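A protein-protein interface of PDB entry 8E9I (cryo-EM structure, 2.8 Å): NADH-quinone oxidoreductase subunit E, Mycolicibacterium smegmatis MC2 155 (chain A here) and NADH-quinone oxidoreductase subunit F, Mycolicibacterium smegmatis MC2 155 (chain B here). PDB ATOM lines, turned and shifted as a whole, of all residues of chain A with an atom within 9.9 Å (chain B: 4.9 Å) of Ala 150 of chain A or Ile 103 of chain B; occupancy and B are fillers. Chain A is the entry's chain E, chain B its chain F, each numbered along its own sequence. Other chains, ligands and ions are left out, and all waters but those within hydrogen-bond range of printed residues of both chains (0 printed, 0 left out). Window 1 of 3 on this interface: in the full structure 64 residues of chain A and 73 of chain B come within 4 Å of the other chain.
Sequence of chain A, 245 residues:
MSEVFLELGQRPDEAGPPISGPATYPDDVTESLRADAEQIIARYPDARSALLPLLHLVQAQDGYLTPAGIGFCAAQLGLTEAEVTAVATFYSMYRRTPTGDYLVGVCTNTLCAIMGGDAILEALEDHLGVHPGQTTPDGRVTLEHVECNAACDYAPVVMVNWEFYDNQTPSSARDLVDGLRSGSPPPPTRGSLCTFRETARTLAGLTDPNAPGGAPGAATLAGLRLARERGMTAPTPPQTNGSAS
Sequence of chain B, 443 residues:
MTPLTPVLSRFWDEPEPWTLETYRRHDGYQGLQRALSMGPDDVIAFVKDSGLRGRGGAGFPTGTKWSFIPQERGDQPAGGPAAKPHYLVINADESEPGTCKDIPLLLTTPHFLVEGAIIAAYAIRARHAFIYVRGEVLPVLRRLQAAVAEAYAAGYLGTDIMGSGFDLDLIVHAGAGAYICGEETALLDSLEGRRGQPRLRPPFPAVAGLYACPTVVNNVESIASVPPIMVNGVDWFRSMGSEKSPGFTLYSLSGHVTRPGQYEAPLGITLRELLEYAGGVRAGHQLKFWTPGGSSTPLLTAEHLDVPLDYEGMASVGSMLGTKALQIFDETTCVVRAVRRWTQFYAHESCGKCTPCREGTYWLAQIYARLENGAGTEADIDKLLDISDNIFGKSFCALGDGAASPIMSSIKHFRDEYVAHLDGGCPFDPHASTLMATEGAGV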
ATOM      1  N   CYS A 107      19.237 -16.228  11.654  1.00  0.00           N
ATOM      2  CA  CYS A 107      18.766 -17.582  11.886  1.00  0.00           C
ATOM      3  C   CYS A 107      19.123 -18.435  10.686  1.00  0.00           C
ATOM      4  O   CYS A 107      18.505 -18.315   9.625  1.00  0.00           O
ATOM      5  CB  CYS A 107      17.263 -17.607  12.122  1.00  0.00           C
ATOM      6  SG  CYS A 107      16.653 -19.264  12.449  1.00  0.00           S
ATOM      7  N   ASN A 109      18.933 -21.715  10.630  1.00  0.00           N
ATOM      8  CA  ASN A 109      18.308 -23.018  10.761  1.00  0.00           C
ATOM      9  C   ASN A 109      17.863 -23.524   9.393  1.00  0.00           C
ATOM     10  O   ASN A 109      17.856 -22.788   8.404  1.00  0.00           O
ATOM     11  CB  ASN A 109      17.118 -22.931  11.713  1.00  0.00           C
ATOM     12  CG  ASN A 109      16.650 -24.280  12.189  1.00  0.00           C
ATOM     13  OD1 ASN A 109      15.675 -24.827  11.678  1.00  0.00           O
ATOM     14  ND2 ASN A 109      17.328 -24.819  13.190  1.00  0.00           N
ATOM     15  N   LEU A 111      14.977 -24.265   7.975  1.00  0.00           N
ATOM     16  CA  LEU A 111      13.906 -23.563   7.280  1.00  0.00           C
ATOM     17  C   LEU A 111      14.328 -22.150   6.898  1.00  0.00           C
ATOM     18  O   LEU A 111      14.287 -21.782   5.720  1.00  0.00           O
ATOM     19  CB  LEU A 111      12.650 -23.543   8.146  1.00  0.00           C
ATOM     20  CG  LEU A 111      11.399 -22.986   7.475  1.00  0.00           C
ATOM     21  CD1 LEU A 111      10.184 -23.705   7.999  1.00  0.00           C
ATOM     22  CD2 LEU A 111      11.265 -21.498   7.713  1.00  0.00           C
ATOM     23  N   CYS A 112      14.771 -21.351   7.869  1.00  0.00           N
ATOM     24  CA  CYS A 112      15.137 -19.972   7.558  1.00  0.00           C
ATOM     25  C   CYS A 112      16.272 -19.917   6.548  1.00  0.00           C
ATOM     26  O   CYS A 112      16.259 -19.083   5.638  1.00  0.00           O
ATOM     27  CB  CYS A 112      15.520 -19.215   8.827  1.00  0.00           C
ATOM     28  SG  CYS A 112      14.162 -18.970   9.973  1.00  0.00           S
ATOM     29  N   VAL A 146      22.334 -18.101  14.350  1.00  0.00           N
ATOM     30  CA  VAL A 146      21.558 -18.664  15.445  1.00  0.00           C
ATOM     31  C   VAL A 146      20.712 -19.807  14.908  1.00  0.00           C
ATOM     32  O   VAL A 146      20.317 -19.802  13.737  1.00  0.00           O
ATOM     33  CB  VAL A 146      20.673 -17.589  16.105  1.00  0.00           C
ATOM     34  CG1 VAL A 146      19.787 -18.202  17.163  1.00  0.00           C
ATOM     35  CG2 VAL A 146      21.533 -16.491  16.696  1.00  0.00           C
ATOM     36  N   GLU A 147      20.437 -20.787  15.764  1.00  0.00           N
ATOM     37  CA  GLU A 147      19.556 -21.884  15.388  1.00  0.00           C
ATOM     38  C   GLU A 147      18.121 -21.382  15.368  1.00  0.00           C
ATOM     39  O   GLU A 147      17.884 -20.180  15.506  1.00  0.00           O
ATOM     40  CB  GLU A 147      19.706 -23.061  16.352  1.00  0.00           C
ATOM     41  N   CYS A 148      17.157 -22.280  15.193  1.00  0.00           N
ATOM     42  CA  CYS A 148      15.772 -21.850  15.092  1.00  0.00           C
ATOM     43  C   CYS A 148      15.394 -20.990  16.285  1.00  0.00           C
ATOM     44  O   CYS A 148      15.648 -21.360  17.434  1.00  0.00           O
ATOM     45  CB  CYS A 148      14.828 -23.045  15.002  1.00  0.00           C
ATOM     46  SG  CYS A 148      13.095 -22.570  14.971  1.00  0.00           S
ATOM     47  N   ASN A 149      14.790 -19.840  16.018  1.00  0.00           N
ATOM     48  CA  ASN A 149      14.340 -18.938  17.061  1.00  0.00           C
ATOM     49  C   ASN A 149      12.838 -19.000  17.278  1.00  0.00           C
ATOM     50  O   ASN A 149      12.276 -18.098  17.906  1.00  0.00           O
ATOM     51  CB  ASN A 149      14.732 -17.508  16.727  1.00  0.00           C
ATOM     52  CG  ASN A 149      14.608 -16.597  17.911  1.00  0.00           C
ATOM     53  OD1 ASN A 149      14.371 -17.042  19.030  1.00  0.00           O
ATOM     54  ND2 ASN A 149      14.697 -15.312  17.665  1.00  0.00           N
ATOM     55  N   ALA A 150      12.174 -20.028  16.766  1.00  0.00           N
ATOM     56  CA  ALA A 150      10.725 -20.135  16.879  1.00  0.00           C
ATOM     57  C   ALA A 150      10.045 -18.895  16.306  1.00  0.00           C
ATOM     58  O   ALA A 150       9.081 -18.377  16.868  1.00  0.00           O
ATOM     59  CB  ALA A 150      10.303 -20.370  18.327  1.00  0.00           C
ATOM     60  N   ALA A 151      10.561 -18.414  15.176  1.00  0.00           N
ATOM     61  CA  ALA A 151       9.904 -17.396  14.367  1.00  0.00           C
ATOM     62  C   ALA A 151       9.873 -17.832  12.909  1.00  0.00           C
ATOM     63  O   ALA A 151      10.095 -17.027  12.004  1.00  0.00           O
ATOM     64  CB  ALA A 151      10.599 -16.045  14.509  1.00  0.00           C
ATOM     65  N   CYS A 152       9.592 -19.113  12.675  1.00  0.00           N
ATOM     66  CA  CYS A 152       9.799 -19.697  11.356  1.00  0.00           C
ATOM     67  C   CYS A 152       8.880 -19.087  10.311  1.00  0.00           C
ATOM     68  O   CYS A 152       9.260 -18.979   9.142  1.00  0.00           O
ATOM     69  CB  CYS A 152       9.591 -21.204  11.435  1.00  0.00           C
ATOM     70  SG  CYS A 152      10.394 -21.928  12.868  1.00  0.00           S
ATOM     71  N   ASP A 153       7.668 -18.690  10.703  1.00  0.00           N
ATOM     72  CA  ASP A 153       6.784 -18.022   9.758  1.00  0.00           C
ATOM     73  C   ASP A 153       7.463 -16.799   9.172  1.00  0.00           C
ATOM     74  O   ASP A 153       7.430 -16.568   7.960  1.00  0.00           O
ATOM     75  CB  ASP A 153       5.492 -17.604  10.445  1.00  0.00           C
ATOM     76  CG  ASP A 153       4.633 -18.770  10.827  1.00  0.00           C
ATOM     77  OD1 ASP A 153       4.701 -19.809  10.145  1.00  0.00           O
ATOM     78  OD2 ASP A 153       3.863 -18.637  11.794  1.00  0.00           O
ATOM     79  N   TYR A 154       8.089 -16.004  10.028  1.00  0.00           N
ATOM     80  CA  TYR A 154       8.753 -14.791   9.591  1.00  0.00           C
ATOM     81  C   TYR A 154      10.107 -15.163   9.016  1.00  0.00           C
ATOM     82  O   TYR A 154      11.153 -14.838   9.583  1.00  0.00           O
ATOM     83  CB  TYR A 154       8.873 -13.818  10.758  1.00  0.00           C
ATOM     84  CG  TYR A 154       7.522 -13.399  11.288  1.00  0.00           C
ATOM     85  CD1 TYR A 154       6.791 -12.404  10.666  1.00  0.00           C
ATOM     86  CD2 TYR A 154       6.974 -14.007  12.404  1.00  0.00           C
ATOM     87  CE1 TYR A 154       5.564 -12.025  11.138  1.00  0.00           C
ATOM     88  CE2 TYR A 154       5.746 -13.631  12.886  1.00  0.00           C
ATOM     89  CZ  TYR A 154       5.047 -12.638  12.249  1.00  0.00           C
ATOM     90  OH  TYR A 154       3.817 -12.252  12.716  1.00  0.00           O
ATOM     91  N   ALA A 155      10.084 -15.817   7.867  1.00  0.00           N
ATOM     92  CA  ALA A 155      11.242 -16.458   7.266  1.00  0.00           C
ATOM     93  C   ALA A 155      12.327 -15.421   7.007  1.00  0.00           C
ATOM     94  O   ALA A 155      12.109 -14.229   7.256  1.00  0.00           O
ATOM     95  CB  ALA A 155      10.821 -17.179   5.989  1.00  0.00           C
ATOM     96  N   VAL A 157      14.369 -14.652   9.156  1.00  0.00           N
ATOM     97  CA  VAL A 157      14.346 -13.833  10.362  1.00  0.00           C
ATOM     98  C   VAL A 157      15.773 -13.481  10.755  1.00  0.00           C
ATOM     99  O   VAL A 157      16.667 -14.335  10.729  1.00  0.00           O
ATOM    100  CB  VAL A 157      13.628 -14.566  11.503  1.00  0.00           C
ATOM    101  CG1 VAL A 157      14.483 -15.701  12.022  1.00  0.00           C
ATOM    102  CG2 VAL A 157      13.300 -13.595  12.626  1.00  0.00           C
ATOM    103  N   MET A 159      17.878 -11.774  13.938  1.00  0.00           N
ATOM    104  CA  MET A 159      17.663 -11.512  15.340  1.00  0.00           C
ATOM    105  C   MET A 159      18.692 -10.450  15.717  1.00  0.00           C
ATOM    106  O   MET A 159      19.805 -10.461  15.191  1.00  0.00           O
ATOM    107  CB  MET A 159      17.903 -12.804  16.115  1.00  0.00           C
ATOM    108  CG  MET A 159      16.673 -13.663  16.344  1.00  0.00           C
ATOM    109  SD  MET A 159      15.116 -12.953  16.909  1.00  0.00           S
ATOM    110  CE  MET A 159      15.595 -12.420  18.523  1.00  0.00           C
ATOM    111  N   TRP A 162      18.431 -10.095  20.549  1.00  0.00           N
ATOM    112  CA  TRP A 162      17.320 -10.982  20.873  1.00  0.00           C
ATOM    113  C   TRP A 162      15.961 -10.331  20.648  1.00  0.00           C
ATOM    114  O   TRP A 162      14.954 -10.815  21.176  1.00  0.00           O
ATOM    115  CB  TRP A 162      17.454 -11.512  22.303  1.00  0.00           C
ATOM    116  CG  TRP A 162      18.774 -12.183  22.511  1.00  0.00           C
ATOM    117  CD1 TRP A 162      19.660 -11.938  23.508  1.00  0.00           C
ATOM    118  CD2 TRP A 162      19.357 -13.212  21.699  1.00  0.00           C
ATOM    119  NE1 TRP A 162      20.764 -12.737  23.367  1.00  0.00           N
ATOM    120  CE2 TRP A 162      20.598 -13.531  22.267  1.00  0.00           C
ATOM    121  CE3 TRP A 162      18.948 -13.895  20.548  1.00  0.00           C
ATOM    122  CZ2 TRP A 162      21.439 -14.494  21.733  1.00  0.00           C
ATOM    123  CZ3 TRP A 162      19.779 -14.854  20.017  1.00  0.00           C
ATOM    124  CH2 TRP A 162      21.014 -15.143  20.610  1.00  0.00           C
ATOM    125  N   GLU A 163      15.910  -9.251  19.872  1.00  0.00           N
ATOM    126  CA  GLU A 163      14.674  -8.803  19.263  1.00  0.00           C
ATOM    127  C   GLU A 163      14.566  -9.381  17.856  1.00  0.00           C
ATOM    128  O   GLU A 163      15.554  -9.830  17.278  1.00  0.00           O
ATOM    129  CB  GLU A 163      14.623  -7.277  19.214  1.00  0.00           C
ATOM    130  N   PHE A 164      13.357  -9.363  17.306  1.00  0.00           N
ATOM    131  CA  PHE A 164      13.080  -9.938  15.995  1.00  0.00           C
ATOM    132  C   PHE A 164      13.222  -8.912  14.884  1.00  0.00           C
ATOM    133  O   PHE A 164      13.012  -7.717  15.093  1.00  0.00           O
ATOM    134  CB  PHE A 164      11.664 -10.519  15.939  1.00  0.00           C
ATOM    135  CG  PHE A 164      11.440 -11.697  16.834  1.00  0.00           C
ATOM    136  CD1 PHE A 164      11.804 -12.962  16.425  1.00  0.00           C
ATOM    137  CD2 PHE A 164      10.840 -11.547  18.067  1.00  0.00           C
ATOM    138  CE1 PHE A 164      11.588 -14.054  17.235  1.00  0.00           C
ATOM    139  CE2 PHE A 164      10.626 -12.639  18.880  1.00  0.00           C
ATOM    140  CZ  PHE A 164      10.999 -13.892  18.462  1.00  0.00           C
ATOM    141  N   ASP A 166      11.597  -9.492  11.078  1.00  0.00           N
ATOM    142  CA  ASP A 166      10.906 -10.466  10.251  1.00  0.00           C
ATOM    143  C   ASP A 166      11.189 -10.245   8.770  1.00  0.00           C
ATOM    144  O   ASP A 166      11.506  -9.139   8.324  1.00  0.00           O
ATOM    145  CB  ASP A 166       9.404 -10.379  10.488  1.00  0.00           C
ATOM    146  CG  ASP A 166       9.038 -10.558  11.938  1.00  0.00           C
ATOM    147  OD1 ASP A 166       9.702 -11.359  12.620  1.00  0.00           O
ATOM    148  OD2 ASP A 166       8.080  -9.901  12.396  1.00  0.00           O
ATOM    149  N   ARG A 190       9.325  -6.863  15.584  1.00  0.00           N
ATOM    150  CA  ARG A 190       8.531  -7.361  16.703  1.00  0.00           C
ATOM    151  C   ARG A 190       9.441  -7.356  17.927  1.00  0.00           C
ATOM    152  O   ARG A 190      10.137  -8.341  18.188  1.00  0.00           O
ATOM    153  CB  ARG A 190       7.990  -8.751  16.398  1.00  0.00           C
ATOM    154  CG  ARG A 190       6.843  -9.180  17.285  1.00  0.00           C
ATOM    155  CD  ARG A 190       6.069 -10.343  16.671  1.00  0.00           C
ATOM    156  NE  ARG A 190       6.809 -11.598  16.733  1.00  0.00           N
ATOM    157  CZ  ARG A 190       7.633 -12.037  15.793  1.00  0.00           C
ATOM    158  NH1 ARG A 190       7.871 -11.339  14.697  1.00  0.00           N
ATOM    159  NH2 ARG A 190       8.234 -13.211  15.957  1.00  0.00           N
ATOM    160  N   GLY A 214       5.989  -4.958  19.830  1.00  0.00           N
ATOM    161  CA  GLY A 214       5.517  -6.326  19.871  1.00  0.00           C
ATOM    162  C   GLY A 214       4.153  -6.549  19.264  1.00  0.00           C
ATOM    163  O   GLY A 214       3.378  -7.353  19.794  1.00  0.00           O
ATOM    164  N   ALA A 215       3.828  -5.865  18.167  1.00  0.00           N
ATOM    165  CA  ALA A 215       2.552  -6.085  17.512  1.00  0.00           C
ATOM    166  C   ALA A 215       2.513  -7.491  16.922  1.00  0.00           C
ATOM    167  O   ALA A 215       3.556  -8.087  16.644  1.00  0.00           O
ATOM    168  CB  ALA A 215       2.322  -5.049  16.417  1.00  0.00           C
ATOM    169  N   PRO A 216       1.317  -8.049  16.730  1.00  0.00           N
ATOM    170  CA  PRO A 216       1.242  -9.443  16.261  1.00  0.00           C
ATOM    171  C   PRO A 216       1.968  -9.693  14.952  1.00  0.00           C
ATOM    172  O   PRO A 216       2.600 -10.746  14.800  1.00  0.00           O
ATOM    173  CB  PRO A 216      -0.268  -9.683  16.129  1.00  0.00           C
ATOM    174  CG  PRO A 216      -0.895  -8.684  17.029  1.00  0.00           C
ATOM    175  CD  PRO A 216      -0.016  -7.476  16.973  1.00  0.00           C
ATOM    176  N   ALA A 219       2.162 -12.818  10.068  1.00  0.00           N
ATOM    177  CA  ALA A 219       2.047 -14.270  10.139  1.00  0.00           C
ATOM    178  C   ALA A 219       1.232 -14.721  11.341  1.00  0.00           C
ATOM    179  O   ALA A 219       0.433 -15.657  11.225  1.00  0.00           O
ATOM    180  CB  ALA A 219       3.429 -14.910  10.177  1.00  0.00           C
ATOM    181  N   THR A 220       1.417 -14.087  12.498  1.00  0.00           N
ATOM    182  CA  THR A 220       0.642 -14.484  13.667  1.00  0.00           C
ATOM    183  C   THR A 220      -0.848 -14.325  13.417  1.00  0.00           C
ATOM    184  O   THR A 220      -1.660 -14.999  14.056  1.00  0.00           O
ATOM    185  CB  THR A 220       1.053 -13.661  14.884  1.00  0.00           C
ATOM    186  OG1 THR A 220       0.836 -12.272  14.616  1.00  0.00           O
ATOM    187  CG2 THR A 220       2.514 -13.887  15.205  1.00  0.00           C
ATOM    188  N   ALA B  92       7.815 -22.813  28.622  1.00  0.00           N
ATOM    189  CA  ALA B  92       7.721 -21.785  27.602  1.00  0.00           C
ATOM    190  C   ALA B  92       8.912 -21.802  26.667  1.00  0.00           C
ATOM    191  O   ALA B  92       8.965 -21.004  25.727  1.00  0.00           O
ATOM    192  CB  ALA B  92       7.579 -20.407  28.248  1.00  0.00           C
ATOM    193  N   GLU B  94      10.592 -22.896  23.528  1.00  0.00           N
ATOM    194  CA  GLU B  94      10.151 -23.424  22.240  1.00  0.00           C
ATOM    195  C   GLU B  94      11.355 -23.324  21.307  1.00  0.00           C
ATOM    196  O   GLU B  94      11.597 -22.282  20.695  1.00  0.00           O
ATOM    197  CB  GLU B  94       8.953 -22.667  21.698  1.00  0.00           C
ATOM    198  CG  GLU B  94       8.348 -23.304  20.468  1.00  0.00           C
ATOM    199  CD  GLU B  94       7.231 -22.481  19.888  1.00  0.00           C
ATOM    200  OE1 GLU B  94       7.434 -21.270  19.682  1.00  0.00           O
ATOM    201  OE2 GLU B  94       6.138 -23.035  19.654  1.00  0.00           O
ATOM    202  N   THR B  99       9.154 -24.800  14.962  1.00  0.00           N
ATOM    203  CA  THR B  99       8.113 -24.626  15.963  1.00  0.00           C
ATOM    204  C   THR B  99       8.048 -23.167  16.381  1.00  0.00           C
ATOM    205  O   THR B  99       8.951 -22.670  17.060  1.00  0.00           O
ATOM    206  CB  THR B  99       8.390 -25.514  17.167  1.00  0.00           C
ATOM    207  OG1 THR B  99       8.766 -26.820  16.719  1.00  0.00           O
ATOM    208  CG2 THR B  99       7.155 -25.621  18.022  1.00  0.00           C
ATOM    209  N   CYS B 100       6.991 -22.479  15.972  1.00  0.00           N
ATOM    210  CA  CYS B 100       6.820 -21.076  16.312  1.00  0.00           C
ATOM    211  C   CYS B 100       5.358 -20.807  16.660  1.00  0.00           C
ATOM    212  O   CYS B 100       4.758 -19.830  16.214  1.00  0.00           O
ATOM    213  CB  CYS B 100       7.310 -20.186  15.171  1.00  0.00           C
ATOM    214  SG  CYS B 100       6.582 -20.550  13.572  1.00  0.00           S
ATOM    215  N   LYS B 101       4.765 -21.688  17.462  1.00  0.00           N
ATOM    216  CA  LYS B 101       3.405 -21.503  17.954  1.00  0.00           C
ATOM    217  C   LYS B 101       3.363 -20.940  19.365  1.00  0.00           C
ATOM    218  O   LYS B 101       2.517 -20.095  19.665  1.00  0.00           O
ATOM    219  CB  LYS B 101       2.643 -22.830  17.919  1.00  0.00           C
ATOM    220  CG  LYS B 101       3.341 -23.974  18.629  1.00  0.00           C
ATOM    221  CD  LYS B 101       2.436 -25.183  18.739  1.00  0.00           C
ATOM    222  CE  LYS B 101       2.982 -26.205  19.717  1.00  0.00           C
ATOM    223  NZ  LYS B 101       2.601 -25.907  21.117  1.00  0.00           N
ATOM    224  N   ASP B 102       4.261 -21.387  20.239  1.00  0.00           N
ATOM    225  CA  ASP B 102       4.310 -20.864  21.598  1.00  0.00           C
ATOM    226  C   ASP B 102       4.729 -19.398  21.619  1.00  0.00           C
ATOM    227  O   ASP B 102       4.180 -18.602  22.383  1.00  0.00           O
ATOM    228  CB  ASP B 102       5.267 -21.704  22.443  1.00  0.00           C
ATOM    229  N   ILE B 103       5.710 -19.025  20.796  1.00  0.00           N
ATOM    230  CA  ILE B 103       6.213 -17.652  20.826  1.00  0.00           C
ATOM    231  C   ILE B 103       5.133 -16.646  20.447  1.00  0.00           C
ATOM    232  O   ILE B 103       4.953 -15.660  21.181  1.00  0.00           O
ATOM    233  CB  ILE B 103       7.473 -17.533  19.950  1.00  0.00           C
ATOM    234  CG1 ILE B 103       8.601 -18.404  20.511  1.00  0.00           C
ATOM    235  CG2 ILE B 103       7.931 -16.089  19.831  1.00  0.00           C
ATOM    236  CD1 ILE B 103       8.989 -18.099  21.933  1.00  0.00           C
ATOM    237  N   PRO B 104       4.408 -16.803  19.337  1.00  0.00           N
ATOM    238  CA  PRO B 104       3.328 -15.846  19.047  1.00  0.00           C
ATOM    239  C   PRO B 104       2.271 -15.797  20.133  1.00  0.00           C
ATOM    240  O   PRO B 104       1.804 -14.712  20.499  1.00  0.00           O
ATOM    241  CB  PRO B 104       2.764 -16.369  17.722  1.00  0.00           C
ATOM    242  CG  PRO B 104       3.893 -17.088  17.102  1.00  0.00           C
ATOM    243  CD  PRO B 104       4.577 -17.766  18.238  1.00  0.00           C
ATOM    244  N   LEU B 105       1.880 -16.956  20.664  1.00  0.00           N
ATOM    245  CA  LEU B 105       0.880 -16.982  21.722  1.00  0.00           C
ATOM    246  C   LEU B 105       1.350 -16.177  22.921  1.00  0.00           C
ATOM    247  O   LEU B 105       0.610 -15.352  23.466  1.00  0.00           O
ATOM    248  CB  LEU B 105       0.586 -18.428  22.119  1.00  0.00           C
ATOM    249  CG  LEU B 105      -0.009 -18.667  23.507  1.00  0.00           C
ATOM    250  CD1 LEU B 105      -1.364 -18.005  23.645  1.00  0.00           C
ATOM    251  CD2 LEU B 105      -0.124 -20.157  23.761  1.00  0.00           C
ATOM    252  N   LEU B 106       2.593 -16.397  23.339  1.00  0.00           N
ATOM    253  CA  LEU B 106       3.115 -15.677  24.491  1.00  0.00           C
ATOM    254  C   LEU B 106       3.186 -14.184  24.214  1.00  0.00           C
ATOM    255  O   LEU B 106       2.818 -13.372  25.068  1.00  0.00           O
ATOM    256  CB  LEU B 106       4.495 -16.217  24.853  1.00  0.00           C
ATOM    257  CG  LEU B 106       4.531 -17.636  25.416  1.00  0.00           C
ATOM    258  CD1 LEU B 106       5.952 -18.016  25.761  1.00  0.00           C
ATOM    259  CD2 LEU B 106       3.636 -17.766  26.629  1.00  0.00           C
ATOM    260  N   LEU B 107       3.647 -13.801  23.023  1.00  0.00           N
ATOM    261  CA  LEU B 107       3.829 -12.383  22.739  1.00  0.00           C
ATOM    262  C   LEU B 107       2.498 -11.649  22.668  1.00  0.00           C
ATOM    263  O   LEU B 107       2.362 -10.550  23.216  1.00  0.00           O
ATOM    264  CB  LEU B 107       4.595 -12.200  21.433  1.00  0.00           C
ATOM    265  CG  LEU B 107       5.157 -10.791  21.282  1.00  0.00           C
ATOM    266  CD1 LEU B 107       6.480 -10.671  22.010  1.00  0.00           C
ATOM    267  CD2 LEU B 107       5.312 -10.433  19.825  1.00  0.00           C
ATOM    268  N   ARG B 134      12.599 -19.782  26.993  1.00  0.00           N
ATOM    269  CA  ARG B 134      13.888 -19.652  26.339  1.00  0.00           C
ATOM    270  C   ARG B 134      14.245 -18.182  26.214  1.00  0.00           C
ATOM    271  O   ARG B 134      13.375 -17.333  26.019  1.00  0.00           O
ATOM    272  CB  ARG B 134      13.841 -20.302  24.957  1.00  0.00           C
ATOM    273  CG  ARG B 134      12.907 -19.593  23.984  1.00  0.00           C
ATOM    274  CD  ARG B 134      12.914 -20.237  22.618  1.00  0.00           C
ATOM    275  NE  ARG B 134      14.237 -20.211  22.009  1.00  0.00           N
ATOM    276  CZ  ARG B 134      14.489 -20.556  20.756  1.00  0.00           C
ATOM    277  NH1 ARG B 134      13.522 -20.923  19.932  1.00  0.00           N
ATOM    278  NH2 ARG B 134      15.743 -20.532  20.319  1.00  0.00           N
ATOM    279  N   VAL B 137      14.157 -14.650  22.841  1.00  0.00           N
ATOM    280  CA  VAL B 137      12.831 -14.216  22.434  1.00  0.00           C
ATOM    281  C   VAL B 137      12.504 -13.001  23.284  1.00  0.00           C
ATOM    282  O   VAL B 137      11.354 -12.790  23.681  1.00  0.00           O
ATOM    283  CB  VAL B 137      11.794 -15.337  22.593  1.00  0.00           C
ATOM    284  CG1 VAL B 137      12.192 -16.524  21.741  1.00  0.00           C
ATOM    285  CG2 VAL B 137      11.670 -15.741  24.044  1.00  0.00           C
ATOM    286  N   VAL B 140       9.229 -11.712  23.894  1.00  0.00           N
ATOM    287  CA  VAL B 140       8.306 -12.602  24.590  1.00  0.00           C
ATOM    288  C   VAL B 140       8.589 -12.604  26.081  1.00  0.00           C
ATOM    289  O   VAL B 140       7.668 -12.659  26.899  1.00  0.00           O
ATOM    290  CB  VAL B 140       8.384 -14.021  24.001  1.00  0.00           C
ATOM    291  CG1 VAL B 140       7.747 -15.026  24.942  1.00  0.00           C
ATOM    292  CG2 VAL B 140       7.702 -14.052  22.659  1.00  0.00           C
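NH2 of Arg 134 of chain B sits at hydrogen-bond distance from O of Cys 148 of chain A, 3.0 Å away.
N of Asp 153 of chain A is in hydrogen-bond range of SG of Cys 100 of chain B.
The backbone NH (N) of Thr 99 of chain B sits close to the side-chain sulfur (SG) of Cys 152 of chain A, 3.8 Å away.
N of Cys 152 of chain A lies within hydrogen-bond range of SG of Cys 100 of chain B.
OE2 of Glu 94 of chain B lies within hydrogen-bond range of N of Lys 101 of chain B (2.9 Å).
The side-chain hydroxyl of Tyr 154 of chain A sits at hydrogen-bond distance from the backbone NH of Thr 220 of chain A, at 3.0 Å.
The side-chain sulfur of Cys 148 of chain A sits close to the backbone NH of Ala 150 of chain A (3.2 Å).
The side-chain carboxylate (OD2) of Asp 166 of chain A is in salt-bridge range of the guanidinium group (NH1) of Arg 190 of chain A, at 2.7 Å.
ND2 of Asn 149 of chain A sits at hydrogen-bond distance from SD of Met 159 of chain A, at 2.5 Å.
The side-chain amide nitrogen (ND2) of Asn 109 of chain A lies close to the backbone NH (N) of Cys 148 of chain A, at 3.2 Å.
Arg 134 of chain B touches Asn 149 of chain A (NH1 to C, 3.3 Å).
OD1 of Asn 149 of chain A touches CG1 of Val 137 of chain B, 3.5 Å away.
CB of Ala 150 of chain A touches OE1 of Glu 94 of chain B, 3.3 Å away.
Ala 150 of chain A touches Thr 99 of chain B.
CB of Cys 100 of chain B touches O of Ala 150 of chain A (3.0 Å).
Ala 150 of chain A touches Ile 103 of chain B.
N of Ala 150 of chain A touches NH1 of Arg 134 of chain B, 3.6 Å away.
Ala 151 of chain A touches Cys 100 of chain B (N to CB, 3.7 Å).
O of Trp 162 of chain A touches C of Val 137 of chain B, 3.9 Å away.
CB of Pro 104 of chain B touches CG2 of Thr 220 of chain A, at 3.5 Å.
Ala 150 of chain A touches just these residues of chain B: Glu 94, Thr 99, Cys 100, Ile 103 and Arg 134.
Of the printed residues of chain A, Ile 103 of chain B touches Ala 150.
Glu 94 of chain B touches just one residue of chain A: Ala 150.
No residue of chain A comes within 4 Å of Asp 102 of chain B.
Of chain A, only Thr 220 (3.5 Å) comes within 4 Å of Pro 104 of chain B.
Printed residues of chain A within 4 Å of Arg 134 of chain B: Cys 148, Asn 149 and Ala 150.
Printed residues of chain A within 4 Å of Leu 107 of chain B: Arg 190 (3.2 Å) and Gly 214 (3.6 Å).
Of the printed residues of chain B, Asp 153 of chain A touches Cys 100.
Cys 112 of chain A touches none of the printed residues of chain B.
The nearest residue of chain B that does not touch Ala 150 of chain A is Pro 104 of chain B (4.7 Å).
The nearest printed residue of chain A that does not touch Ile 103 of chain B is Phe 164 of chain A (4.01 Å).
Of the 26 printed residues of chain A, 10 touch a printed residue of chain B.
Of the 14 printed residues of chain B, 8 touch a printed residue of chain A.
Among the printed residues, 16 pairs touch across the chains.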
